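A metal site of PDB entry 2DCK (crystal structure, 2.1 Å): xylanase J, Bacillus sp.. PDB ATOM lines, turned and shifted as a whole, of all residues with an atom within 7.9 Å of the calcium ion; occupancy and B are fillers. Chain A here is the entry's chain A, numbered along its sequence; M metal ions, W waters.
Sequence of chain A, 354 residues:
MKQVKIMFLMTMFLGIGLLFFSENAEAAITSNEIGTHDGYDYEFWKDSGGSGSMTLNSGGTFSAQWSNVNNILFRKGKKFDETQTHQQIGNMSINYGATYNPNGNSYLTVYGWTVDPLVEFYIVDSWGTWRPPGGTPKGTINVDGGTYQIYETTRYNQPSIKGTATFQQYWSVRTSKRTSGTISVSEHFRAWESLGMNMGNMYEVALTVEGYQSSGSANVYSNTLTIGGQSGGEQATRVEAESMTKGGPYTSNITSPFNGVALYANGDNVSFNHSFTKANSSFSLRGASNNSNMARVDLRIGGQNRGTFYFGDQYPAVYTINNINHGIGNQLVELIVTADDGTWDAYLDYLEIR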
ATOM      1  N   TYR A 250      -0.551 -24.642  16.652  1.00  0.00           N
ATOM      2  CA  TYR A 250      -0.335 -25.947  17.240  1.00  0.00           C
ATOM      3  C   TYR A 250      -1.322 -26.374  18.303  1.00  0.00           C
ATOM      4  O   TYR A 250      -1.219 -27.447  18.764  1.00  0.00           O
ATOM      5  CB  TYR A 250       1.034 -26.001  17.881  1.00  0.00           C
ATOM      6  CG  TYR A 250       2.190 -25.799  16.942  1.00  0.00           C
ATOM      7  CD1 TYR A 250       2.493 -26.737  15.930  1.00  0.00           C
ATOM      8  CD2 TYR A 250       3.041 -24.702  17.117  1.00  0.00           C
ATOM      9  CE1 TYR A 250       3.574 -26.530  15.115  1.00  0.00           C
ATOM     10  CE2 TYR A 250       4.116 -24.522  16.321  1.00  0.00           C
ATOM     11  CZ  TYR A 250       4.361 -25.406  15.313  1.00  0.00           C
ATOM     12  OH  TYR A 250       5.450 -25.143  14.544  1.00  0.00           O
ATOM     13  N   LEU A 263      -1.434 -24.886  24.654  1.00  0.00           N
ATOM     14  CA  LEU A 263      -1.048 -23.759  23.819  1.00  0.00           C
ATOM     15  C   LEU A 263       0.424 -23.751  23.866  1.00  0.00           C
ATOM     16  O   LEU A 263       1.006 -23.626  24.905  1.00  0.00           O
ATOM     17  CB  LEU A 263      -1.642 -22.495  24.386  1.00  0.00           C
ATOM     18  CG  LEU A 263      -3.113 -22.452  24.670  1.00  0.00           C
ATOM     19  CD1 LEU A 263      -3.483 -21.018  25.120  1.00  0.00           C
ATOM     20  CD2 LEU A 263      -3.990 -22.841  23.445  1.00  0.00           C
ATOM     21  N   TYR A 264       1.075 -24.070  22.751  1.00  0.00           N
ATOM     22  CA  TYR A 264       2.472 -24.292  22.693  1.00  0.00           C
ATOM     23  C   TYR A 264       3.262 -23.080  22.258  1.00  0.00           C
ATOM     24  O   TYR A 264       4.439 -22.911  22.704  1.00  0.00           O
ATOM     25  CB  TYR A 264       2.759 -25.426  21.671  1.00  0.00           C
ATOM     26  CG  TYR A 264       2.122 -26.750  21.981  1.00  0.00           C
ATOM     27  CD1 TYR A 264       2.745 -27.705  22.789  1.00  0.00           C
ATOM     28  CD2 TYR A 264       0.914 -27.049  21.482  1.00  0.00           C
ATOM     29  CE1 TYR A 264       2.120 -28.952  23.065  1.00  0.00           C
ATOM     30  CE2 TYR A 264       0.295 -28.260  21.767  1.00  0.00           C
ATOM     31  CZ  TYR A 264       0.897 -29.194  22.539  1.00  0.00           C
ATOM     32  OH  TYR A 264       0.163 -30.351  22.720  1.00  0.00           O
ATOM     33  N   ALA A 265       2.721 -22.320  21.308  1.00  0.00           N
ATOM     34  CA  ALA A 265       3.493 -21.243  20.677  1.00  0.00           C
ATOM     35  C   ALA A 265       2.744 -19.917  20.679  1.00  0.00           C
ATOM     36  O   ALA A 265       1.508 -19.844  20.927  1.00  0.00           O
ATOM     37  CB  ALA A 265       3.882 -21.606  19.265  1.00  0.00           C
ATOM     38  N   ASN A 266       3.489 -18.829  20.448  1.00  0.00           N
ATOM     39  CA  ASN A 266       2.809 -17.534  20.274  1.00  0.00           C
ATOM     40  C   ASN A 266       1.744 -17.628  19.220  1.00  0.00           C
ATOM     41  O   ASN A 266       1.970 -18.191  18.166  1.00  0.00           O
ATOM     42  CB  ASN A 266       3.764 -16.392  20.053  1.00  0.00           C
ATOM     43  CG  ASN A 266       4.642 -16.098  21.292  1.00  0.00           C
ATOM     44  OD1 ASN A 266       5.790 -15.699  21.162  1.00  0.00           O
ATOM     45  ND2 ASN A 266       4.156 -16.451  22.456  1.00  0.00           N
ATOM     46  N   ASP A 268      -1.018 -19.474  19.557  1.00  0.00           N
ATOM     47  CA  ASP A 268      -1.967 -20.510  20.014  1.00  0.00           C
ATOM     48  C   ASP A 268      -3.008 -19.924  20.898  1.00  0.00           C
ATOM     49  O   ASP A 268      -2.710 -19.211  21.843  1.00  0.00           O
ATOM     50  CB  ASP A 268      -1.265 -21.689  20.685  1.00  0.00           C
ATOM     51  CG  ASP A 268      -0.531 -22.584  19.681  1.00  0.00           C
ATOM     52  OD1 ASP A 268      -0.802 -22.469  18.443  1.00  0.00           O
ATOM     53  OD2 ASP A 268       0.385 -23.406  20.019  1.00  0.00           O
ATOM     54  N   ASN A 290       3.612 -26.953  31.584  1.00  0.00           N
ATOM     55  CA  ASN A 290       4.116 -28.276  31.312  1.00  0.00           C
ATOM     56  C   ASN A 290       5.320 -28.674  32.148  1.00  0.00           C
ATOM     57  O   ASN A 290       5.639 -29.853  32.237  1.00  0.00           O
ATOM     58  CB  ASN A 290       4.499 -28.468  29.836  1.00  0.00           C
ATOM     59  CG  ASN A 290       5.752 -27.731  29.458  1.00  0.00           C
ATOM     60  OD1 ASN A 290       6.667 -28.256  28.750  1.00  0.00           O
ATOM     61  ND2 ASN A 290       5.821 -26.526  29.862  1.00  0.00           N
ATOM     62  N   VAL A 337      -1.531 -17.398  24.056  1.00  0.00           N
ATOM     63  CA  VAL A 337      -0.162 -17.256  24.429  1.00  0.00           C
ATOM     64  C   VAL A 337       0.554 -16.194  23.600  1.00  0.00           C
ATOM     65  O   VAL A 337       0.481 -16.263  22.373  1.00  0.00           O
ATOM     66  CB  VAL A 337       0.513 -18.608  24.302  1.00  0.00           C
ATOM     67  CG1 VAL A 337       2.059 -18.516  24.392  1.00  0.00           C
ATOM     68  CG2 VAL A 337       0.004 -19.528  25.471  1.00  0.00           C
ATOM     69  N   ALA A 339       3.822 -14.848  25.278  1.00  0.00           N
ATOM     70  CA  ALA A 339       5.153 -14.773  25.829  1.00  0.00           C
ATOM     71  C   ALA A 339       5.958 -16.067  25.711  1.00  0.00           C
ATOM     72  O   ALA A 339       6.950 -16.206  26.335  1.00  0.00           O
ATOM     73  CB  ALA A 339       5.065 -14.372  27.239  1.00  0.00           C
ATOM     74  N   ASP A 340       5.565 -17.007  24.871  1.00  0.00           N
ATOM     75  CA  ASP A 340       6.361 -18.194  24.710  1.00  0.00           C
ATOM     76  C   ASP A 340       7.784 -17.930  24.207  1.00  0.00           C
ATOM     77  O   ASP A 340       7.977 -17.085  23.355  1.00  0.00           O
ATOM     78  CB  ASP A 340       5.660 -19.133  23.768  1.00  0.00           C
ATOM     79  CG  ASP A 340       6.510 -20.352  23.372  1.00  0.00           C
ATOM     80  OD1 ASP A 340       6.653 -21.268  24.250  1.00  0.00           O
ATOM     81  OD2 ASP A 340       7.036 -20.457  22.222  1.00  0.00           O
ATOM     82  N   ASP A 341       8.750 -18.710  24.688  1.00  0.00           N
ATOM     83  CA  ASP A 341      10.131 -18.584  24.253  1.00  0.00           C
ATOM     84  C   ASP A 341      10.790 -19.948  24.153  1.00  0.00           C
ATOM     85  O   ASP A 341      12.006 -20.038  24.103  1.00  0.00           O
ATOM     86  CB  ASP A 341      10.917 -17.653  25.184  1.00  0.00           C
ATOM     87  CG  ASP A 341      11.155 -18.260  26.539  1.00  0.00           C
ATOM     88  OD1 ASP A 341      11.892 -17.651  27.372  1.00  0.00           O
ATOM     89  OD2 ASP A 341      10.607 -19.367  26.854  1.00  0.00           O
ATOM     90  N   GLY A 342      10.012 -20.999  24.045  1.00  0.00           N
ATOM     91  CA  GLY A 342      10.542 -22.346  23.796  1.00  0.00           C
ATOM     92  C   GLY A 342      10.905 -23.017  25.122  1.00  0.00           C
ATOM     93  O   GLY A 342      11.559 -24.024  25.067  1.00  0.00           O
ATOM     94  N   THR A 343      10.513 -22.444  26.263  1.00  0.00           N
ATOM     95  CA  THR A 343      10.795 -23.077  27.548  1.00  0.00           C
ATOM     96  C   THR A 343       9.629 -23.600  28.335  1.00  0.00           C
ATOM     97  O   THR A 343       9.861 -24.129  29.422  1.00  0.00           O
ATOM     98  CB  THR A 343      11.577 -22.085  28.480  1.00  0.00           C
ATOM     99  OG1 THR A 343      10.766 -20.914  28.747  1.00  0.00           O
ATOM    100  CG2 THR A 343      12.917 -21.605  27.772  1.00  0.00           C
ATOM    101  N   TRP A 344       8.400 -23.399  27.881  1.00  0.00           N
ATOM    102  CA  TRP A 344       7.203 -23.892  28.510  1.00  0.00           C
ATOM    103  C   TRP A 344       6.017 -23.929  27.550  1.00  0.00           C
ATOM    104  O   TRP A 344       6.036 -23.247  26.500  1.00  0.00           O
ATOM    105  CB  TRP A 344       6.832 -23.044  29.754  1.00  0.00           C
ATOM    106  CG  TRP A 344       6.713 -21.569  29.527  1.00  0.00           C
ATOM    107  CD1 TRP A 344       7.679 -20.626  29.828  1.00  0.00           C
ATOM    108  CD2 TRP A 344       5.578 -20.816  29.007  1.00  0.00           C
ATOM    109  NE1 TRP A 344       7.244 -19.376  29.506  1.00  0.00           N
ATOM    110  CE2 TRP A 344       5.964 -19.448  29.006  1.00  0.00           C
ATOM    111  CE3 TRP A 344       4.310 -21.149  28.529  1.00  0.00           C
ATOM    112  CZ2 TRP A 344       5.166 -18.438  28.543  1.00  0.00           C
ATOM    113  CZ3 TRP A 344       3.486 -20.120  28.052  1.00  0.00           C
ATOM    114  CH2 TRP A 344       3.929 -18.787  28.058  1.00  0.00           C
ATOM    115  N   ASP A 345       5.008 -24.706  27.887  1.00  0.00           N
ATOM    116  CA  ASP A 345       3.734 -24.655  27.238  1.00  0.00           C
ATOM    117  C   ASP A 345       2.686 -24.381  28.312  1.00  0.00           C
ATOM    118  O   ASP A 345       2.930 -24.643  29.509  1.00  0.00           O
ATOM    119  CB  ASP A 345       3.431 -26.003  26.584  1.00  0.00           C
ATOM    120  CG  ASP A 345       4.465 -26.389  25.561  1.00  0.00           C
ATOM    121  OD1 ASP A 345       4.850 -27.601  25.450  1.00  0.00           O
ATOM    122  OD2 ASP A 345       4.944 -25.522  24.812  1.00  0.00           O
ATOM    123  N   ALA A 346       1.522 -23.881  27.898  1.00  0.00           N
ATOM    124  CA  ALA A 346       0.416 -23.666  28.805  1.00  0.00           C
ATOM    125  C   ALA A 346      -0.664 -24.713  28.574  1.00  0.00           C
ATOM    126  O   ALA A 346      -1.088 -24.952  27.468  1.00  0.00           O
ATOM    127  CB  ALA A 346      -0.150 -22.285  28.620  1.00  0.00           C
HETATM  128 CA    CA M   1       6.096 -23.571  24.067  1.00  0.00          CA
HETATM  129  O   HOH W   1       7.748 -23.220  21.880  1.00  0.00           O
HETATM  130  O   HOH W   2       8.103 -25.042  24.565  1.00  0.00           O
HETATM  131  O   HOH W   3       6.435 -25.585  22.362  1.00  0.00           O
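Within 4 Å of the calcium ion: Tyr 264, Asp 340, Trp 344 and Asp 345.
N of Tyr 264 lies within hydrogen-bond range of OD2 of Asp 268, at 2.9 Å.
The side-chain carboxylate (OD1) of Asp 340 sits close to the backbone NH (N) of Gly 342, 3.4 Å away.
The backbone NH of Asp 340 sits close to the side-chain amide nitrogen of Asn 266 (2.9 Å).
The backbone NH of Asp 345 lies close to the side-chain amide nitrogen of Asn 290, at 2.8 Å.
The backbone carbonyl oxygen (O) of Tyr 264 binds the calcium ion (2.2 Å).
OD1 of Asp 340 is bound to the calcium ion (2.4 Å).
The side-chain carboxylate (OD2) of Asp 345 binds the calcium ion (2.4 Å).
O of Trp 344 binds the calcium ion (2.5 Å).
The calcium ion is bound by water W2 (2.5 Å).
Water W3 is bound to the calcium ion (2.7 Å).
Water W1 binds the calcium ion (2.8 Å).
The calcium ion has seven donor atoms within binding distance.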
